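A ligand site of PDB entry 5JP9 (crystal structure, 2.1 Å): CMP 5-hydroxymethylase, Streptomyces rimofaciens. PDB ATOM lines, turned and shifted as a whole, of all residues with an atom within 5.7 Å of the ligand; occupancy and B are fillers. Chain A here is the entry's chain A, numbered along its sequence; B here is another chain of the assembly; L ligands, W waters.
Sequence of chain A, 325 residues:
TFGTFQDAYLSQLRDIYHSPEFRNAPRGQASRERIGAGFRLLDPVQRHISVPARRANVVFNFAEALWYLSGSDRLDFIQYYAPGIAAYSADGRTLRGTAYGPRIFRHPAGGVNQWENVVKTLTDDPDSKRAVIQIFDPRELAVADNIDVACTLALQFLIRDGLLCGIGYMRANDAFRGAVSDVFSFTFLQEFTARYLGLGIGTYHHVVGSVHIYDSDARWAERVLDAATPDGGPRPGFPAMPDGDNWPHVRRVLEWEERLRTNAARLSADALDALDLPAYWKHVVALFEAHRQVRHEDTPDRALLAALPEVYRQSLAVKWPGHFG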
ATOM      1  N   PRO A  26      34.984  19.220 -24.070  1.00  0.00           N
ATOM      2  CA  PRO A  26      35.347  20.100 -22.947  1.00  0.00           C
ATOM      3  C   PRO A  26      34.902  19.473 -21.632  1.00  0.00           C
ATOM      4  O   PRO A  26      33.770  19.022 -21.492  1.00  0.00           O
ATOM      5  CB  PRO A  26      34.570  21.390 -23.236  1.00  0.00           C
ATOM      6  CG  PRO A  26      34.111  21.285 -24.664  1.00  0.00           C
ATOM      7  CD  PRO A  26      33.944  19.816 -24.929  1.00  0.00           C
ATOM      8  N   ARG A  27      35.820  19.460 -20.658  1.00  0.00           N
ATOM      9  CA  ARG A  27      35.587  18.821 -19.349  1.00  0.00           C
ATOM     10  C   ARG A  27      35.055  17.399 -19.508  1.00  0.00           C
ATOM     11  O   ARG A  27      34.231  16.934 -18.706  1.00  0.00           O
ATOM     12  CB  ARG A  27      34.649  19.683 -18.491  1.00  0.00           C
ATOM     13  CG  ARG A  27      35.204  21.091 -18.209  1.00  0.00           C
ATOM     14  CD  ARG A  27      34.471  21.811 -17.059  1.00  0.00           C
ATOM     15  NE  ARG A  27      33.079  22.125 -17.378  1.00  0.00           N
ATOM     16  CZ  ARG A  27      32.017  21.642 -16.737  1.00  0.00           C
ATOM     17  NH1 ARG A  27      32.175  20.816 -15.715  1.00  0.00           N
ATOM     18  NH2 ARG A  27      30.796  22.009 -17.103  1.00  0.00           N
ATOM     19  N   GLU A  64      12.430  30.094 -14.126  1.00  0.00           N
ATOM     20  CA  GLU A  64      13.815  30.550 -14.236  1.00  0.00           C
ATOM     21  C   GLU A  64      13.877  32.063 -14.350  1.00  0.00           C
ATOM     22  O   GLU A  64      14.679  32.712 -13.670  1.00  0.00           O
ATOM     23  CB  GLU A  64      14.508  29.913 -15.449  1.00  0.00           C
ATOM     24  CG  GLU A  64      15.990  30.250 -15.552  1.00  0.00           C
ATOM     25  CD  GLU A  64      16.618  29.860 -16.878  1.00  0.00           C
ATOM     26  OE1 GLU A  64      17.295  28.812 -16.901  1.00  0.00           O
ATOM     27  OE2 GLU A  64      16.450  30.603 -17.875  1.00  0.00           O
ATOM     28  N   TYR A  68      15.495  34.652 -11.479  1.00  0.00           N
ATOM     29  CA  TYR A  68      16.431  35.749 -11.725  1.00  0.00           C
ATOM     30  C   TYR A  68      15.914  37.065 -11.134  1.00  0.00           C
ATOM     31  O   TYR A  68      16.643  37.789 -10.454  1.00  0.00           O
ATOM     32  CB  TYR A  68      16.683  35.941 -13.231  1.00  0.00           C
ATOM     33  CG  TYR A  68      17.360  34.807 -13.961  1.00  0.00           C
ATOM     34  CD1 TYR A  68      18.016  33.776 -13.276  1.00  0.00           C
ATOM     35  CD2 TYR A  68      17.375  34.784 -15.349  1.00  0.00           C
ATOM     36  CE1 TYR A  68      18.630  32.730 -13.958  1.00  0.00           C
ATOM     37  CE2 TYR A  68      17.988  33.757 -16.045  1.00  0.00           C
ATOM     38  CZ  TYR A  68      18.608  32.732 -15.349  1.00  0.00           C
ATOM     39  OH  TYR A  68      19.220  31.724 -16.069  1.00  0.00           O
ATOM     40  N   THR A  98      25.270  29.440 -12.423  1.00  0.00           N
ATOM     41  CA  THR A  98      23.909  29.279 -12.955  1.00  0.00           C
ATOM     42  C   THR A  98      22.934  30.344 -12.436  1.00  0.00           C
ATOM     43  O   THR A  98      21.932  30.634 -13.101  1.00  0.00           O
ATOM     44  CB  THR A  98      23.405  27.854 -12.637  1.00  0.00           C
ATOM     45  OG1 THR A  98      24.237  26.895 -13.302  1.00  0.00           O
ATOM     46  CG2 THR A  98      21.965  27.626 -13.094  1.00  0.00           C
ATOM     47  N   TYR A 100      21.843  33.701 -12.243  1.00  0.00           N
ATOM     48  CA  TYR A 100      22.031  35.041 -12.799  1.00  0.00           C
ATOM     49  C   TYR A 100      21.377  36.138 -11.951  1.00  0.00           C
ATOM     50  O   TYR A 100      21.734  37.303 -12.087  1.00  0.00           O
ATOM     51  CB  TYR A 100      21.487  35.096 -14.231  1.00  0.00           C
ATOM     52  CG  TYR A 100      22.245  34.193 -15.238  1.00  0.00           C
ATOM     53  CD1 TYR A 100      23.497  33.682 -14.950  1.00  0.00           C
ATOM     54  CD2 TYR A 100      21.683  33.900 -16.477  1.00  0.00           C
ATOM     55  CE1 TYR A 100      24.180  32.876 -15.880  1.00  0.00           C
ATOM     56  CE2 TYR A 100      22.352  33.100 -17.398  1.00  0.00           C
ATOM     57  CZ  TYR A 100      23.583  32.590 -17.099  1.00  0.00           C
ATOM     58  OH  TYR A 100      24.229  31.811 -18.022  1.00  0.00           O
ATOM     59  N   VAL A 149      30.459  27.552 -13.571  1.00  0.00           N
ATOM     60  CA  VAL A 149      31.010  28.833 -14.018  1.00  0.00           C
ATOM     61  C   VAL A 149      30.013  29.472 -14.977  1.00  0.00           C
ATOM     62  O   VAL A 149      29.562  28.823 -15.934  1.00  0.00           O
ATOM     63  CB  VAL A 149      32.375  28.647 -14.705  1.00  0.00           C
ATOM     64  CG1 VAL A 149      32.906  29.972 -15.311  1.00  0.00           C
ATOM     65  CG2 VAL A 149      33.381  28.011 -13.756  1.00  0.00           C
ATOM     66  N   CYS A 151      28.181  31.016 -17.914  1.00  0.00           N
ATOM     67  CA  CYS A 151      28.438  30.981 -19.339  1.00  0.00           C
ATOM     68  C   CYS A 151      27.917  32.216 -20.075  1.00  0.00           C
ATOM     69  O   CYS A 151      28.214  32.379 -21.262  1.00  0.00           O
ATOM     70  CB  CYS A 151      27.935  29.659 -19.923  1.00  0.00           C
ATOM     71  SG  CYS A 151      26.188  29.488 -20.043  1.00  0.00           S
ATOM     72  N   THR A 152      27.146  33.081 -19.416  1.00  0.00           N
ATOM     73  CA  THR A 152      26.738  34.354 -20.010  1.00  0.00           C
ATOM     74  C   THR A 152      27.745  35.427 -19.625  1.00  0.00           C
ATOM     75  O   THR A 152      28.107  35.566 -18.453  1.00  0.00           O
ATOM     76  CB  THR A 152      25.331  34.734 -19.559  1.00  0.00           C
ATOM     77  OG1 THR A 152      24.435  33.685 -19.952  1.00  0.00           O
ATOM     78  CG2 THR A 152      24.858  36.084 -20.164  1.00  0.00           C
ATOM     79  N   MET A 170      27.309  35.438 -24.833  1.00  0.00           N
ATOM     80  CA  MET A 170      27.659  34.256 -24.049  1.00  0.00           C
ATOM     81  C   MET A 170      28.967  33.664 -24.551  1.00  0.00           C
ATOM     82  O   MET A 170      29.266  33.689 -25.745  1.00  0.00           O
ATOM     83  CB  MET A 170      26.573  33.159 -24.082  1.00  0.00           C
ATOM     84  CG  MET A 170      25.133  33.667 -23.804  1.00  0.00           C
ATOM     85  SD  MET A 170      23.941  32.333 -23.954  1.00  0.00           S
ATOM     86  CE  MET A 170      24.282  31.406 -22.453  1.00  0.00           C
ATOM     87  N   ARG A 171      29.763  33.142 -23.605  1.00  0.00           N
ATOM     88  CA  ARG A 171      30.972  32.425 -23.970  1.00  0.00           C
ATOM     89  C   ARG A 171      30.657  31.022 -24.485  1.00  0.00           C
ATOM     90  O   ARG A 171      31.466  30.453 -25.228  1.00  0.00           O
ATOM     91  CB  ARG A 171      31.928  32.331 -22.769  1.00  0.00           C
ATOM     92  CG  ARG A 171      31.399  31.485 -21.597  1.00  0.00           C
ATOM     93  CD  ARG A 171      32.472  31.210 -20.490  1.00  0.00           C
ATOM     94  NE  ARG A 171      31.875  30.431 -19.398  1.00  0.00           N
ATOM     95  CZ  ARG A 171      31.668  29.114 -19.434  1.00  0.00           C
ATOM     96  NH1 ARG A 171      32.051  28.410 -20.503  1.00  0.00           N
ATOM     97  NH2 ARG A 171      31.082  28.489 -18.420  1.00  0.00           N
ATOM     98  N   ALA A 172      29.511  30.465 -24.093  1.00  0.00           N
ATOM     99  CA  ALA A 172      29.124  29.119 -24.493  1.00  0.00           C
ATOM    100  C   ALA A 172      27.623  28.949 -24.287  1.00  0.00           C
ATOM    101  O   ALA A 172      27.034  29.569 -23.399  1.00  0.00           O
ATOM    102  CB  ALA A 172      29.884  28.051 -23.684  1.00  0.00           C
ATOM    103  N   ASN A 173      27.018  28.086 -25.110  1.00  0.00           N
ATOM    104  CA  ASN A 173      25.581  27.875 -25.021  1.00  0.00           C
ATOM    105  C   ASN A 173      25.281  26.471 -25.516  1.00  0.00           C
ATOM    106  O   ASN A 173      25.727  26.077 -26.591  1.00  0.00           O
ATOM    107  CB  ASN A 173      24.838  28.928 -25.849  1.00  0.00           C
ATOM    108  CG  ASN A 173      23.393  29.128 -25.456  1.00  0.00           C
ATOM    109  OD1 ASN A 173      22.629  29.742 -26.217  1.00  0.00           O
ATOM    110  ND2 ASN A 173      23.007  28.664 -24.264  1.00  0.00           N
ATOM    111  N   ASP A 174      24.560  25.708 -24.697  1.00  0.00           N
ATOM    112  CA  ASP A 174      24.037  24.423 -25.113  1.00  0.00           C
ATOM    113  C   ASP A 174      22.880  24.701 -26.055  1.00  0.00           C
ATOM    114  O   ASP A 174      21.828  25.179 -25.633  1.00  0.00           O
ATOM    115  CB  ASP A 174      23.598  23.636 -23.883  1.00  0.00           C
ATOM    116  CG  ASP A 174      22.677  22.461 -24.192  1.00  0.00           C
ATOM    117  OD1 ASP A 174      22.574  22.029 -25.352  1.00  0.00           O
ATOM    118  OD2 ASP A 174      22.080  21.948 -23.238  1.00  0.00           O
ATOM    119  N   GLY A 178      19.954  24.476 -23.086  1.00  0.00           N
ATOM    120  CA  GLY A 178      20.152  25.770 -22.425  1.00  0.00           C
ATOM    121  C   GLY A 178      19.638  26.950 -23.243  1.00  0.00           C
ATOM    122  O   GLY A 178      19.085  27.897 -22.678  1.00  0.00           O
ATOM    123  N   ALA A 179      19.841  26.915 -24.555  1.00  0.00           N
ATOM    124  CA  ALA A 179      19.418  28.023 -25.414  1.00  0.00           C
ATOM    125  C   ALA A 179      17.923  28.289 -25.315  1.00  0.00           C
ATOM    126  O   ALA A 179      17.495  29.445 -25.400  1.00  0.00           O
ATOM    127  CB  ALA A 179      19.796  27.729 -26.869  1.00  0.00           C
ATOM    128  N   ASP A 182      17.591  30.078 -21.959  1.00  0.00           N
ATOM    129  CA  ASP A 182      18.368  31.324 -21.941  1.00  0.00           C
ATOM    130  C   ASP A 182      17.709  32.408 -22.787  1.00  0.00           C
ATOM    131  O   ASP A 182      17.553  33.543 -22.340  1.00  0.00           O
ATOM    132  CB  ASP A 182      19.793  31.075 -22.426  1.00  0.00           C
ATOM    133  CG  ASP A 182      20.602  30.229 -21.474  1.00  0.00           C
ATOM    134  OD1 ASP A 182      20.377  30.308 -20.241  1.00  0.00           O
ATOM    135  OD2 ASP A 182      21.444  29.461 -21.980  1.00  0.00           O
ATOM    136  N   SER A 210      31.003  29.465 -28.025  1.00  0.00           N
ATOM    137  CA  SER A 210      30.866  28.048 -28.361  1.00  0.00           C
ATOM    138  C   SER A 210      29.404  27.653 -28.259  1.00  0.00           C
ATOM    139  O   SER A 210      28.865  27.538 -27.163  1.00  0.00           O
ATOM    140  CB  SER A 210      31.712  27.173 -27.426  1.00  0.00           C
ATOM    141  OG  SER A 210      31.295  25.820 -27.469  1.00  0.00           O
ATOM    142  N   HIS A 212      26.828  24.493 -28.975  1.00  0.00           N
ATOM    143  CA  HIS A 212      27.158  23.073 -29.053  1.00  0.00           C
ATOM    144  C   HIS A 212      25.959  22.187 -28.743  1.00  0.00           C
ATOM    145  O   HIS A 212      24.989  22.606 -28.101  1.00  0.00           O
ATOM    146  CB  HIS A 212      28.330  22.747 -28.104  1.00  0.00           C
ATOM    147  CG  HIS A 212      28.162  23.275 -26.707  1.00  0.00           C
ATOM    148  ND1 HIS A 212      28.669  24.499 -26.320  1.00  0.00           N
ATOM    149  CD2 HIS A 212      27.540  22.756 -25.619  1.00  0.00           C
ATOM    150  CE1 HIS A 212      28.370  24.706 -25.045  1.00  0.00           C
ATOM    151  NE2 HIS A 212      27.683  23.662 -24.594  1.00  0.00           N
ATOM    152  N   TYR A 214      25.510  18.397 -27.017  1.00  0.00           N
ATOM    153  CA  TYR A 214      26.150  17.261 -26.364  1.00  0.00           C
ATOM    154  C   TYR A 214      25.745  15.964 -27.057  1.00  0.00           C
ATOM    155  O   TYR A 214      24.584  15.787 -27.431  1.00  0.00           O
ATOM    156  CB  TYR A 214      25.778  17.207 -24.878  1.00  0.00           C
ATOM    157  CG  TYR A 214      26.067  18.511 -24.172  1.00  0.00           C
ATOM    158  CD1 TYR A 214      27.363  19.024 -24.116  1.00  0.00           C
ATOM    159  CD2 TYR A 214      25.050  19.240 -23.593  1.00  0.00           C
ATOM    160  CE1 TYR A 214      27.637  20.225 -23.503  1.00  0.00           C
ATOM    161  CE2 TYR A 214      25.312  20.450 -22.951  1.00  0.00           C
ATOM    162  CZ  TYR A 214      26.599  20.932 -22.919  1.00  0.00           C
ATOM    163  OH  TYR A 214      26.851  22.132 -22.305  1.00  0.00           O
ATOM    164  N   LYS B 129      35.755  25.684 -22.831  1.00  0.00           N
ATOM    165  CA  LYS B 129      34.890  26.795 -23.218  1.00  0.00           C
ATOM    166  C   LYS B 129      34.930  27.949 -22.233  1.00  0.00           C
ATOM    167  O   LYS B 129      34.218  28.942 -22.442  1.00  0.00           O
ATOM    168  CB  LYS B 129      33.455  26.309 -23.355  1.00  0.00           C
ATOM    169  CG  LYS B 129      33.236  25.292 -24.460  1.00  0.00           C
ATOM    170  CD  LYS B 129      31.890  24.618 -24.334  1.00  0.00           C
ATOM    171  CE  LYS B 129      31.767  23.779 -23.075  1.00  0.00           C
ATOM    172  NZ  LYS B 129      30.432  23.094 -22.989  1.00  0.00           N
ATOM    173  N   ARG B 130      35.729  27.839 -21.166  1.00  0.00           N
ATOM    174  CA  ARG B 130      35.740  28.778 -20.050  1.00  0.00           C
ATOM    175  C   ARG B 130      36.879  29.775 -20.104  1.00  0.00           C
ATOM    176  O   ARG B 130      37.006  30.598 -19.185  1.00  0.00           O
ATOM    177  CB  ARG B 130      35.815  28.013 -18.720  1.00  0.00           C
ATOM    178  CG  ARG B 130      34.606  27.143 -18.413  1.00  0.00           C
ATOM    179  CD  ARG B 130      34.922  26.237 -17.209  1.00  0.00           C
ATOM    180  NE  ARG B 130      33.731  25.639 -16.625  1.00  0.00           N
ATOM    181  CZ  ARG B 130      33.733  24.992 -15.465  1.00  0.00           C
ATOM    182  NH1 ARG B 130      34.870  24.858 -14.782  1.00  0.00           N
ATOM    183  NH2 ARG B 130      32.607  24.485 -14.970  1.00  0.00           N
HETATM  184  N1  LIG L   1      24.737  26.273 -20.119  1.00  0.00           N
HETATM  185  C1  LIG L   1      23.812  27.062 -20.965  1.00  0.00           C
HETATM  186  N2  LIG L   1      22.969  28.079 -20.330  1.00  0.00           N
HETATM  187  C2  LIG L   1      22.999  28.307 -18.888  1.00  0.00           C
HETATM  188  C3  LIG L   1      23.910  27.524 -18.033  1.00  0.00           C
HETATM  189  C4  LIG L   1      24.776  26.484 -18.674  1.00  0.00           C
HETATM  190  O1  LIG L   1      23.773  26.868 -22.149  1.00  0.00           O
HETATM  191  N3  LIG L   1      22.149  29.323 -18.314  1.00  0.00           N
HETATM  192  C5  LIG L   1      25.582  25.237 -20.730  1.00  0.00           C
HETATM  193  C6  LIG L   1      26.671  25.845 -21.709  1.00  0.00           C
HETATM  194  C7  LIG L   1      27.992  25.585 -21.010  1.00  0.00           C
HETATM  195  C8  LIG L   1      27.759  24.551 -20.170  1.00  0.00           C
HETATM  196  O2  LIG L   1      26.233  24.677 -19.741  1.00  0.00           O
HETATM  197  O3  LIG L   1      29.012  25.239 -22.022  1.00  0.00           O
HETATM  198  C9  LIG L   1      28.567  24.682 -18.922  1.00  0.00           C
HETATM  199  O4  LIG L   1      29.790  24.043 -19.129  1.00  0.00           O
HETATM  200  P1  LIG L   1      31.147  24.949 -19.276  1.00  0.00           P
HETATM  201  O5  LIG L   1      31.051  25.823 -20.502  1.00  0.00           O
HETATM  202  O6  LIG L   1      32.303  23.991 -19.454  1.00  0.00           O
HETATM  203  O7  LIG L   1      31.356  25.766 -18.014  1.00  0.00           O
HETATM  204  O   HOH W   1      31.287  21.576 -20.732  1.00  0.00           O
HETATM  205  O   HOH W   2      30.127  25.534 -15.684  1.00  0.00           O
HETATM  206  O   HOH W   3      25.666  30.078 -16.542  1.00  0.00           O
HETATM  207  O   HOH W   4      27.259  27.752 -16.913  1.00  0.00           O
HETATM  208  O   HOH W   5      20.464  26.024 -18.773  1.00  0.00           O
HETATM  209  O   HOH W   6      34.579  24.155 -20.734  1.00  0.00           O
HETATM  210  O   HOH W   7      21.183  30.015 -15.627  1.00  0.00           O
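NZ of Lys 129 of chain B is in salt-bridge range of O5 of the ligand, at 3.7 Å. The backbone NH (N) of Asp 174 is in hydrogen-bond range of an oxygen (O1) of the ligand, 2.9 Å away. OD2 of Asp 182 is in hydrogen-bond range of N2 of the ligand (2.6 Å). A ring nitrogen (NE2) of His 212 sits close to an oxygen (O3) of the ligand (3.3 Å). NE of Arg 27 lies within salt-bridge range of O6 of the ligand, 2.9 Å away. The side-chain hydroxyl (OH) of Tyr 100 is in hydrogen-bond range of a nitrogen (N3) of the ligand, at 3.3 Å. ND2 of Asn 173 is in hydrogen-bond range of O1 of the ligand, 2.9 Å away. The guanidinium group (NE) of Arg 130 of chain B lies within salt-bridge range of an oxygen (O7) of the ligand. An oxygen (O7) of the ligand is in salt-bridge range of the guanidinium group (NH2) of Arg 171. N2 of the ligand lies close to SG of Cys 151 (3.5 Å).
SD of Met 170 sits close to OD1 of Asn 173 (3.7 Å). A ring nitrogen (NE2) of His 212 lies within hydrogen-bond range of the side-chain hydroxyl (OH) of Tyr 214 (2.9 Å). The side-chain hydroxyl (OG1) of Thr 152 is in hydrogen-bond range of the side-chain hydroxyl (OH) of Tyr 100 (2.7 Å). A ring nitrogen (ND1) of His 212 is in hydrogen-bond range of the side-chain hydroxyl of Ser 210 (3.2 Å). The guanidinium group (NH2) of Arg 171 is in hydrogen-bond range of the backbone carbonyl oxygen (O) of Val 149 (2.9 Å). The backbone carbonyl oxygen (O) of Asp 174 is in hydrogen-bond range of the backbone NH (N) of Ala 179 (2.9 Å). The backbone NH (N) of His 212 sits at hydrogen-bond distance from the backbone carbonyl oxygen (O) of Asn 173. OD2 of Asp 182 is in hydrogen-bond range of ND2 of Asn 173, 2.9 Å away.
Merely in contact with the ligand: Tyr 214, Ala 172 and Gly 178. Within 4 Å of the ligand: Arg 27, Tyr 100, Cys 151, Arg 171, Ala 172, Asn 173, Asp 174, Gly 178, Asp 182, His 212, Tyr 214, Lys 129 of chain B and Arg 130 of chain B. The nearest printed residue that does not touch the ligand is Val 149 (4.1 Å).
Water W6 bridges O6 of the ligand (2.6 Å) and N of Lys 129 of chain B (2.8 Å). Water W2 lies within hydrogen-bond range of O7 of the ligand, NH2 of Arg 130 of chain B and N of Val 149. Water W1 bridges NZ of Lys 129 of chain B (2.9 Å) and O6 of the ligand (2.9 Å). Water W7 lies within hydrogen-bond range of OH of Tyr 68 (2.6 Å), O of Thr 98 (2.7 Å) and N3 of the ligand (2.9 Å). Water W4 lies within hydrogen-bond range of the backbone carbonyl oxygen (O) of Val 149 (2.7 Å) and the side-chain sulfur (SG) of Cys 151 (3.7 Å). Water W3 bridges the side-chain hydroxyl of Tyr 100 (2.7 Å) and the backbone NH of Cys 151 (3.0 Å).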
